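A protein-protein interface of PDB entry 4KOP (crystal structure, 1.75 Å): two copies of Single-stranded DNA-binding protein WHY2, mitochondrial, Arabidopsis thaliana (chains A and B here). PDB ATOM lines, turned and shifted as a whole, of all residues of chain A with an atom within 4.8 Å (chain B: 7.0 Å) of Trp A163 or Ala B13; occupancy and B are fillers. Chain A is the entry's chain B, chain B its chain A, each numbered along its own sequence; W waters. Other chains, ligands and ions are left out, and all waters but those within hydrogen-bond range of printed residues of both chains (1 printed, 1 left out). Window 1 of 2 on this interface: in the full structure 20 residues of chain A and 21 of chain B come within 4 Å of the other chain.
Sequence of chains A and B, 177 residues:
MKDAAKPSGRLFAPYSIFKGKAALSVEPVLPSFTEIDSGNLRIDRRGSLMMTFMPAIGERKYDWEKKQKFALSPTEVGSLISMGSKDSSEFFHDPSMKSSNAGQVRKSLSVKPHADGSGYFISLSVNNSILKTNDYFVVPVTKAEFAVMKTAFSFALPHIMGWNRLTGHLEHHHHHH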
ATOM      1  N   PHE A  33      26.605  21.587  22.429  1.00  0.00           N
ATOM      2  CA  PHE A  33      26.286  21.507  21.030  1.00  0.00           C
ATOM      3  C   PHE A  33      27.592  21.274  20.280  1.00  0.00           C
ATOM      4  O   PHE A  33      28.603  21.906  20.573  1.00  0.00           O
ATOM      5  CB  PHE A  33      25.678  22.807  20.496  1.00  0.00           C
ATOM      6  CG  PHE A  33      24.236  23.032  20.894  1.00  0.00           C
ATOM      7  CD1 PHE A  33      23.929  23.615  22.105  1.00  0.00           C
ATOM      8  CD2 PHE A  33      23.206  22.678  20.036  1.00  0.00           C
ATOM      9  CE1 PHE A  33      22.590  23.870  22.453  1.00  0.00           C
ATOM     10  CE2 PHE A  33      21.873  22.926  20.381  1.00  0.00           C
ATOM     11  CZ  PHE A  33      21.590  23.519  21.614  1.00  0.00           C
ATOM     12  N   ILE A  43      22.933  18.513  19.827  1.00  0.00           N
ATOM     13  CA  ILE A  43      23.338  18.287  21.202  1.00  0.00           C
ATOM     14  C   ILE A  43      24.025  16.930  21.397  1.00  0.00           C
ATOM     15  O   ILE A  43      23.425  15.870  21.147  1.00  0.00           O
ATOM     16  CB  ILE A  43      22.110  18.399  22.149  1.00  0.00           C
ATOM     17  CG1 ILE A  43      21.605  19.841  22.138  1.00  0.00           C
ATOM     18  CG2 ILE A  43      22.490  17.957  23.521  1.00  0.00           C
ATOM     19  CD1 ILE A  43      20.418  20.151  23.053  1.00  0.00           C
ATOM     20  N   PRO A 158      14.385  26.098  29.578  1.00  0.00           N
ATOM     21  CA  PRO A 158      14.723  26.290  28.155  1.00  0.00           C
ATOM     22  C   PRO A 158      16.234  26.350  27.904  1.00  0.00           C
ATOM     23  O   PRO A 158      16.650  26.004  26.821  1.00  0.00           O
ATOM     24  CB  PRO A 158      14.053  27.624  27.798  1.00  0.00           C
ATOM     25  CG  PRO A 158      13.126  27.912  28.897  1.00  0.00           C
ATOM     26  CD  PRO A 158      13.605  27.223  30.111  1.00  0.00           C
ATOM     27  N   MET A 161      17.415  22.726  27.888  1.00  0.00           N
ATOM     28  CA  MET A 161      16.905  22.099  26.693  1.00  0.00           C
ATOM     29  C   MET A 161      17.585  22.628  25.410  1.00  0.00           C
ATOM     30  O   MET A 161      17.397  22.049  24.337  1.00  0.00           O
ATOM     31  CB  MET A 161      15.408  22.401  26.548  1.00  0.00           C
ATOM     32  CG  MET A 161      14.526  21.774  27.608  1.00  0.00           C
ATOM     33  SD  MET A 161      12.860  22.452  27.555  1.00  0.00           S
ATOM     34  CE  MET A 161      12.210  21.753  26.016  1.00  0.00           C
ATOM     35  N   GLY A 162      18.346  23.716  25.524  1.00  0.00           N
ATOM     36  CA  GLY A 162      19.029  24.302  24.397  1.00  0.00           C
ATOM     37  C   GLY A 162      18.199  25.275  23.599  1.00  0.00           C
ATOM     38  O   GLY A 162      18.618  25.792  22.550  1.00  0.00           O
ATOM     39  N   TRP A 163      16.993  25.555  24.075  1.00  0.00           N
ATOM     40  CA  TRP A 163      16.111  26.456  23.341  1.00  0.00           C
ATOM     41  C   TRP A 163      16.532  27.914  23.345  1.00  0.00           C
ATOM     42  O   TRP A 163      16.155  28.671  22.448  1.00  0.00           O
ATOM     43  CB  TRP A 163      14.649  26.311  23.830  1.00  0.00           C
ATOM     44  CG  TRP A 163      13.966  25.038  23.296  1.00  0.00           C
ATOM     45  CD1 TRP A 163      14.535  23.846  22.989  1.00  0.00           C
ATOM     46  CD2 TRP A 163      12.555  24.881  23.037  1.00  0.00           C
ATOM     47  NE1 TRP A 163      13.579  22.956  22.548  1.00  0.00           N
ATOM     48  CE2 TRP A 163      12.350  23.568  22.592  1.00  0.00           C
ATOM     49  CE3 TRP A 163      11.456  25.728  23.173  1.00  0.00           C
ATOM     50  CZ2 TRP A 163      11.073  23.091  22.216  1.00  0.00           C
ATOM     51  CZ3 TRP A 163      10.213  25.266  22.802  1.00  0.00           C
ATOM     52  CH2 TRP A 163      10.024  23.948  22.340  1.00  0.00           C
ATOM     53  N   ASN A 164      17.312  28.323  24.320  1.00  0.00           N
ATOM     54  CA  ASN A 164      17.888  29.670  24.269  1.00  0.00           C
ATOM     55  C   ASN A 164      18.776  29.879  23.058  1.00  0.00           C
ATOM     56  O   ASN A 164      18.860  30.981  22.528  1.00  0.00           O
ATOM     57  CB  ASN A 164      18.666  30.009  25.528  1.00  0.00           C
ATOM     58  CG  ASN A 164      19.863  29.133  25.699  1.00  0.00           C
ATOM     59  OD1 ASN A 164      19.760  27.921  25.586  1.00  0.00           O
ATOM     60  ND2 ASN A 164      21.036  29.740  25.854  1.00  0.00           N
ATOM     61  N   ARG A 165      19.452  28.821  22.638  1.00  0.00           N
ATOM     62  CA  ARG A 165      20.299  28.860  21.452  1.00  0.00           C
ATOM     63  C   ARG A 165      19.505  28.908  20.174  1.00  0.00           C
ATOM     64  O   ARG A 165      19.973  29.412  19.169  1.00  0.00           O
ATOM     65  CB  ARG A 165      21.237  27.648  21.432  1.00  0.00           C
ATOM     66  CG  ARG A 165      22.080  27.517  22.689  1.00  0.00           C
ATOM     67  CD  ARG A 165      23.251  28.499  22.744  1.00  0.00           C
ATOM     68  NE  ARG A 165      24.105  28.349  21.561  1.00  0.00           N
ATOM     69  CZ  ARG A 165      25.148  27.529  21.488  1.00  0.00           C
ATOM     70  NH1 ARG A 165      25.484  26.766  22.526  1.00  0.00           N
ATOM     71  NH2 ARG A 165      25.856  27.465  20.377  1.00  0.00           N
ATOM     72  N   LEU A 166      18.293  28.365  20.183  1.00  0.00           N
ATOM     73  CA  LEU A 166      17.467  28.373  18.981  1.00  0.00           C
ATOM     74  C   LEU A 166      16.876  29.753  18.781  1.00  0.00           C
ATOM     75  O   LEU A 166      16.769  30.243  17.674  1.00  0.00           O
ATOM     76  CB  LEU A 166      16.358  27.319  19.063  1.00  0.00           C
ATOM     77  CG  LEU A 166      16.778  25.895  19.392  1.00  0.00           C
ATOM     78  CD1 LEU A 166      15.545  24.978  19.487  1.00  0.00           C
ATOM     79  CD2 LEU A 166      17.771  25.346  18.394  1.00  0.00           C
ATOM     80  N   THR A 167      16.507  30.395  19.877  1.00  0.00           N
ATOM     81  CA  THR A 167      15.793  31.655  19.821  1.00  0.00           C
ATOM     82  C   THR A 167      16.776  32.801  19.838  1.00  0.00           C
ATOM     83  O   THR A 167      16.399  33.936  19.575  1.00  0.00           O
ATOM     84  CB  THR A 167      14.848  31.835  21.020  1.00  0.00           C
ATOM     85  OG1 THR A 167      15.614  31.729  22.227  1.00  0.00           O
ATOM     86  CG2 THR A 167      13.731  30.807  21.001  1.00  0.00           C
ATOM     87  N   ARG B  10      22.375  25.865  11.117  1.00  0.00           N
ATOM     88  CA  ARG B  10      21.194  25.485  11.896  1.00  0.00           C
ATOM     89  C   ARG B  10      21.601  24.659  13.121  1.00  0.00           C
ATOM     90  O   ARG B  10      22.294  23.638  13.001  1.00  0.00           O
ATOM     91  CB  ARG B  10      20.185  24.729  10.995  1.00  0.00           C
ATOM     92  CG  ARG B  10      19.081  23.867  11.679  1.00  0.00           C
ATOM     93  CD  ARG B  10      17.843  24.654  12.070  1.00  0.00           C
ATOM     94  NE  ARG B  10      16.625  23.829  12.045  1.00  0.00           N
ATOM     95  CZ  ARG B  10      15.919  23.435  13.110  1.00  0.00           C
ATOM     96  NH1 ARG B  10      16.279  23.786  14.348  1.00  0.00           N
ATOM     97  NH2 ARG B  10      14.821  22.688  12.928  1.00  0.00           N
ATOM     98  N   LEU B  11      21.163  25.134  14.287  1.00  0.00           N
ATOM     99  CA  LEU B  11      21.200  24.382  15.542  1.00  0.00           C
ATOM    100  C   LEU B  11      19.887  23.616  15.672  1.00  0.00           C
ATOM    101  O   LEU B  11      18.827  24.119  15.292  1.00  0.00           O
ATOM    102  CB  LEU B  11      21.365  25.337  16.723  1.00  0.00           C
ATOM    103  CG  LEU B  11      22.781  25.767  17.120  1.00  0.00           C
ATOM    104  CD1 LEU B  11      23.437  26.588  16.025  1.00  0.00           C
ATOM    105  CD2 LEU B  11      22.766  26.533  18.425  1.00  0.00           C
ATOM    106  N   PHE B  12      19.962  22.378  16.118  1.00  0.00           N
ATOM    107  CA  PHE B  12      18.768  21.567  16.349  1.00  0.00           C
ATOM    108  C   PHE B  12      18.734  21.316  17.842  1.00  0.00           C
ATOM    109  O   PHE B  12      19.724  20.869  18.398  1.00  0.00           O
ATOM    110  CB  PHE B  12      18.845  20.193  15.674  1.00  0.00           C
ATOM    111  CG  PHE B  12      18.859  20.225  14.158  1.00  0.00           C
ATOM    112  CD1 PHE B  12      20.050  20.360  13.464  1.00  0.00           C
ATOM    113  CD2 PHE B  12      17.684  20.102  13.436  1.00  0.00           C
ATOM    114  CE1 PHE B  12      20.061  20.386  12.044  1.00  0.00           C
ATOM    115  CE2 PHE B  12      17.685  20.123  12.032  1.00  0.00           C
ATOM    116  CZ  PHE B  12      18.879  20.270  11.341  1.00  0.00           C
ATOM    117  N   ALA B  13      17.600  21.546  18.477  1.00  0.00           N
ATOM    118  CA  ALA B  13      17.419  21.142  19.886  1.00  0.00           C
ATOM    119  C   ALA B  13      15.930  20.825  20.203  1.00  0.00           C
ATOM    120  O   ALA B  13      15.316  21.427  21.125  1.00  0.00           O
ATOM    121  CB  ALA B  13      17.948  22.220  20.819  1.00  0.00           C
ATOM    122  N   PRO B  14      15.380  19.839  19.505  1.00  0.00           N
ATOM    123  CA  PRO B  14      13.968  19.529  19.760  1.00  0.00           C
ATOM    124  C   PRO B  14      13.791  18.901  21.135  1.00  0.00           C
ATOM    125  O   PRO B  14      14.741  18.337  21.715  1.00  0.00           O
ATOM    126  CB  PRO B  14      13.626  18.523  18.654  1.00  0.00           C
ATOM    127  CG  PRO B  14      14.937  17.852  18.338  1.00  0.00           C
ATOM    128  CD  PRO B  14      15.953  18.965  18.452  1.00  0.00           C
ATOM    129  N   TYR B  15      12.607  19.065  21.673  1.00  0.00           N
ATOM    130  CA  TYR B  15      12.156  18.306  22.823  1.00  0.00           C
ATOM    131  C   TYR B  15      11.391  17.144  22.242  1.00  0.00           C
ATOM    132  O   TYR B  15      10.415  17.334  21.486  1.00  0.00           O
ATOM    133  CB  TYR B  15      11.279  19.126  23.727  1.00  0.00           C
ATOM    134  CG  TYR B  15      10.749  18.358  24.936  1.00  0.00           C
ATOM    135  CD1 TYR B  15      11.620  17.734  25.835  1.00  0.00           C
ATOM    136  CD2 TYR B  15       9.388  18.235  25.148  1.00  0.00           C
ATOM    137  CE1 TYR B  15      11.145  17.058  26.965  1.00  0.00           C
ATOM    138  CE2 TYR B  15       8.883  17.577  26.254  1.00  0.00           C
ATOM    139  CZ  TYR B  15       9.754  16.970  27.171  1.00  0.00           C
ATOM    140  OH  TYR B  15       9.255  16.294  28.267  1.00  0.00           O
ATOM    141  N   SER B  16      11.866  15.936  22.537  1.00  0.00           N
ATOM    142  CA  SER B  16      11.305  14.732  21.926  1.00  0.00           C
ATOM    143  C   SER B  16      10.774  13.723  22.960  1.00  0.00           C
ATOM    144  O   SER B  16      11.389  13.518  24.019  1.00  0.00           O
ATOM    145  CB  SER B  16      12.373  14.052  21.059  1.00  0.00           C
ATOM    146  OG  SER B  16      12.792  14.894  20.006  1.00  0.00           O
ATOM    147  N   VAL B  26       9.156  18.525  19.272  1.00  0.00           N
ATOM    148  CA  VAL B  26       8.654  19.886  19.166  1.00  0.00           C
ATOM    149  C   VAL B  26       9.843  20.831  19.246  1.00  0.00           C
ATOM    150  O   VAL B  26      10.774  20.590  20.000  1.00  0.00           O
ATOM    151  CB  VAL B  26       7.611  20.212  20.256  1.00  0.00           C
ATOM    152  CG1 VAL B  26       6.394  19.251  20.122  1.00  0.00           C
ATOM    153  CG2 VAL B  26       8.185  20.103  21.654  1.00  0.00           C
ATOM    154  N   GLU B  27       9.786  21.881  18.438  1.00  0.00           N
ATOM    155  CA  GLU B  27      10.887  22.838  18.319  1.00  0.00           C
ATOM    156  C   GLU B  27      10.355  24.147  17.748  1.00  0.00           C
ATOM    157  O   GLU B  27       9.549  24.123  16.832  1.00  0.00           O
ATOM    158  CB  GLU B  27      11.930  22.229  17.372  1.00  0.00           C
ATOM    159  CG  GLU B  27      13.304  22.759  17.541  1.00  0.00           C
ATOM    160  CD  GLU B  27      14.294  22.121  16.560  1.00  0.00           C
ATOM    161  OE1 GLU B  27      13.859  21.490  15.562  1.00  0.00           O
ATOM    162  OE2 GLU B  27      15.492  22.279  16.795  1.00  0.00           O
ATOM    163  N   PRO B  28      10.843  25.294  18.241  1.00  0.00           N
ATOM    164  CA  PRO B  28      10.437  26.581  17.650  1.00  0.00           C
ATOM    165  C   PRO B  28      11.055  26.788  16.293  1.00  0.00           C
ATOM    166  O   PRO B  28      12.154  26.279  16.047  1.00  0.00           O
ATOM    167  CB  PRO B  28      10.944  27.627  18.648  1.00  0.00           C
ATOM    168  CG  PRO B  28      12.027  26.966  19.390  1.00  0.00           C
ATOM    169  CD  PRO B  28      11.735  25.472  19.395  1.00  0.00           C
ATOM    170  N   LEU B  49       5.579  26.996  16.137  1.00  0.00           N
ATOM    171  CA  LEU B  49       6.063  25.923  17.000  1.00  0.00           C
ATOM    172  C   LEU B  49       5.813  24.648  16.193  1.00  0.00           C
ATOM    173  O   LEU B  49       4.641  24.251  15.982  1.00  0.00           O
ATOM    174  CB  LEU B  49       5.325  25.900  18.348  1.00  0.00           C
ATOM    175  CG  LEU B  49       5.924  25.018  19.433  1.00  0.00           C
ATOM    176  CD1 LEU B  49       5.961  23.521  19.043  1.00  0.00           C
ATOM    177  CD2 LEU B  49       7.310  25.483  19.833  1.00  0.00           C
ATOM    178  N   VAL B 148       6.696  20.603  30.600  1.00  0.00           N
ATOM    179  CA  VAL B 148       7.859  21.021  29.797  1.00  0.00           C
ATOM    180  C   VAL B 148       7.388  21.787  28.566  1.00  0.00           C
ATOM    181  O   VAL B 148       7.917  22.850  28.239  1.00  0.00           O
ATOM    182  CB  VAL B 148       8.752  19.834  29.353  1.00  0.00           C
ATOM    183  CG1 VAL B 148       9.855  20.296  28.423  1.00  0.00           C
ATOM    184  CG2 VAL B 148       9.351  19.114  30.604  1.00  0.00           C
ATOM    185  N   MET B 149       6.388  21.242  27.879  1.00  0.00           N
ATOM    186  CA  MET B 149       5.884  21.895  26.669  1.00  0.00           C
ATOM    187  C   MET B 149       5.325  23.279  27.006  1.00  0.00           C
ATOM    188  O   MET B 149       5.678  24.255  26.380  1.00  0.00           O
ATOM    189  CB  MET B 149       4.862  21.025  25.965  1.00  0.00           C
ATOM    190  CG  MET B 149       5.445  19.782  25.373  1.00  0.00           C
ATOM    191  SD  MET B 149       4.160  18.812  24.557  1.00  0.00           S
ATOM    192  CE  MET B 149       5.096  17.415  24.017  1.00  0.00           C
ATOM    193  N   THR B 151       5.995  25.310  29.504  1.00  0.00           N
ATOM    194  CA  THR B 151       7.074  26.205  29.925  1.00  0.00           C
ATOM    195  C   THR B 151       7.952  26.603  28.737  1.00  0.00           C
ATOM    196  O   THR B 151       8.275  27.783  28.535  1.00  0.00           O
ATOM    197  CB  THR B 151       7.945  25.549  31.000  1.00  0.00           C
ATOM    198  OG1 THR B 151       7.149  25.226  32.166  1.00  0.00           O
ATOM    199  CG2 THR B 151       9.034  26.472  31.390  1.00  0.00           C
ATOM    200  N   ALA B 152       8.377  25.622  27.960  1.00  0.00           N
ATOM    201  CA  ALA B 152       9.231  25.884  26.799  1.00  0.00           C
ATOM    202  C   ALA B 152       8.504  26.681  25.731  1.00  0.00           C
ATOM    203  O   ALA B 152       9.078  27.592  25.114  1.00  0.00           O
ATOM    204  CB  ALA B 152       9.747  24.618  26.231  1.00  0.00           C
ATOM    205  N   PHE B 153       7.232  26.352  25.526  1.00  0.00           N
ATOM    206  CA  PHE B 153       6.424  27.060  24.537  1.00  0.00           C
ATOM    207  C   PHE B 153       6.245  28.510  24.973  1.00  0.00           C
ATOM    208  O   PHE B 153       6.300  29.421  24.142  1.00  0.00           O
ATOM    209  CB  PHE B 153       5.030  26.446  24.342  1.00  0.00           C
ATOM    210  CG  PHE B 153       5.013  25.100  23.636  1.00  0.00           C
ATOM    211  CD1 PHE B 153       6.182  24.410  23.338  1.00  0.00           C
ATOM    212  CD2 PHE B 153       3.801  24.507  23.295  1.00  0.00           C
ATOM    213  CE1 PHE B 153       6.142  23.211  22.759  1.00  0.00           C
ATOM    214  CE2 PHE B 153       3.773  23.272  22.680  1.00  0.00           C
ATOM    215  CZ  PHE B 153       4.925  22.629  22.411  1.00  0.00           C
ATOM    216  N   SER B 154       5.988  28.731  26.250  1.00  0.00           N
ATOM    217  CA  SER B 154       5.863  30.092  26.766  1.00  0.00           C
ATOM    218  C   SER B 154       7.151  30.887  26.556  1.00  0.00           C
ATOM    219  O   SER B 154       7.118  32.072  26.213  1.00  0.00           O
ATOM    220  CB  SER B 154       5.480  30.111  28.249  1.00  0.00           C
ATOM    221  OG  SER B 154       4.174  29.631  28.439  1.00  0.00           O
ATOM    222  N   PHE B 155       8.284  30.252  26.829  1.00  0.00           N
ATOM    223  CA  PHE B 155       9.580  30.889  26.596  1.00  0.00           C
ATOM    224  C   PHE B 155       9.725  31.275  25.116  1.00  0.00           C
ATOM    225  O   PHE B 155      10.181  32.377  24.791  1.00  0.00           O
ATOM    226  CB  PHE B 155      10.686  29.911  26.979  1.00  0.00           C
ATOM    227  CG  PHE B 155      12.048  30.356  26.538  1.00  0.00           C
ATOM    228  CD1 PHE B 155      12.744  31.250  27.312  1.00  0.00           C
ATOM    229  CD2 PHE B 155      12.607  29.929  25.322  1.00  0.00           C
ATOM    230  CE1 PHE B 155      13.995  31.713  26.930  1.00  0.00           C
ATOM    231  CE2 PHE B 155      13.839  30.394  24.926  1.00  0.00           C
ATOM    232  CZ  PHE B 155      14.534  31.288  25.737  1.00  0.00           C
ATOM    233  N   ALA B 156       9.374  30.361  24.219  1.00  0.00           N
ATOM    234  CA  ALA B 156       9.608  30.541  22.786  1.00  0.00           C
ATOM    235  C   ALA B 156       8.646  31.540  22.139  1.00  0.00           C
ATOM    236  O   ALA B 156       8.994  32.167  21.136  1.00  0.00           O
ATOM    237  CB  ALA B 156       9.545  29.204  22.036  1.00  0.00           C
ATOM    238  N   LEU B 157       7.441  31.639  22.693  1.00  0.00           N
ATOM    239  CA  LEU B 157       6.345  32.399  22.049  1.00  0.00           C
ATOM    240  C   LEU B 157       6.724  33.828  21.626  1.00  0.00           C
ATOM    241  O   LEU B 157       6.518  34.192  20.484  1.00  0.00           O
ATOM    242  CB  LEU B 157       5.113  32.417  22.941  1.00  0.00           C
ATOM    243  CG  LEU B 157       3.882  33.090  22.345  1.00  0.00           C
ATOM    244  CD1 LEU B 157       3.554  32.521  21.011  1.00  0.00           C
ATOM    245  CD2 LEU B 157       2.718  32.893  23.270  1.00  0.00           C
ATOM    246  N   HIS B 159       9.564  34.972  20.958  1.00  0.00           N
ATOM    247  CA  HIS B 159      10.573  34.870  19.896  1.00  0.00           C
ATOM    248  C   HIS B 159       9.977  34.478  18.538  1.00  0.00           C
ATOM    249  O   HIS B 159      10.347  35.020  17.477  1.00  0.00           O
ATOM    250  CB  HIS B 159      11.633  33.873  20.341  1.00  0.00           C
ATOM    251  CG  HIS B 159      12.366  34.331  21.546  1.00  0.00           C
ATOM    252  ND1 HIS B 159      13.228  35.405  21.511  1.00  0.00           N
ATOM    253  CD2 HIS B 159      12.333  33.912  22.830  1.00  0.00           C
ATOM    254  CE1 HIS B 159      13.713  35.613  22.723  1.00  0.00           C
ATOM    255  NE2 HIS B 159      13.182  34.720  23.543  1.00  0.00           N
HETATM  256  O   HOH W   1      20.233  18.366  19.146  1.00  0.00           O
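No position is printed for both chains. Of the 22 pairs that touch across the chains among the printed residues, none has its exchanged pair printed and touching as well.
Of chain A, only Phe A33, Ile A43, Met A161, Trp A163 and Leu A166 come within 4 Å of Ala B13. Printed residues of chain B within 4 Å of Ile A43: Ala B13 (3.9 Å). Of the printed residues of chain A, Val B26 touches Trp A163. Printed residues of chain A within 4 Å of Phe B153: Trp A163 (3.97 Å). Of the printed residues of chain A, Glu B27 touches Trp A163 and Leu A166. Ser B16 touches none of the printed residues of chain A. The nearest printed residue of chain B that does not touch Trp A163 is Leu B49 (4.001 Å). The nearest residue of chain A that does not touch Ala B13 is Gly A162 (4.03 Å).
Of the 21 printed residues of chain B, 12 touch a printed residue of chain A. Along chain B the printed residues that touch a printed residue of chain A span positions 11 to 159. Among the printed residues, 22 pairs touch across the chains. Among the printed residues, no Asp or Glu carboxylate lies within 4 Å of a Lys or Arg side-chain nitrogen of the other chain.
The backbone carbonyl oxygen (O) of Ala B13 sits at hydrogen-bond distance from the indole nitrogen (NE1) of Trp A163 (2.7 Å).
The guanidinium group (NH1) of Arg B10 is in salt-bridge range of the side-chain carboxylate (OE2) of Glu B27 (3.0 Å). The side-chain carboxylate (OE2) of Glu B27 sits at hydrogen-bond distance from the backbone NH (N) of Ala B13 (2.8 Å). N of Val B26 is in hydrogen-bond range of O of Tyr B15, 2.8 Å away. The backbone carbonyl oxygen (O) of Pro A158 is in hydrogen-bond range of the backbone NH (N) of Trp A163 (2.8 Å). The backbone carbonyl oxygen (O) of Pro A158 sits at hydrogen-bond distance from the backbone NH (N) of Asn A164 (3.5 Å). O of Trp A163 is in hydrogen-bond range of OG1 of Thr A167 (3.1 Å).
Water W1 lies within hydrogen-bond range of O of Phe B12 and N of Ile A43.
Among the printed residues, pairs that only touch across the chains: Phe A33 with Phe B12, Phe A33 with Ala B13, Ile A43 with Ala B13, Pro A158 with Phe B155, Met A161 with Ala B13, Met A161 with Tyr B15, Met A161 with Val B148, Met A161 with Ala B152, Trp A163 with Val B26, Trp A163 with Glu B27, Trp A163 with Pro B28, Trp A163 with Ala B152, Trp A163 with Phe B153, Trp A163 with Phe B155, Arg A165 with Leu B11, Leu A166 with Leu B11, Leu A166 with Ala B13, Leu A166 with Glu B27, Leu A166 with Pro B28, Thr A167 with Phe B155 and Thr A167 with His B159.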
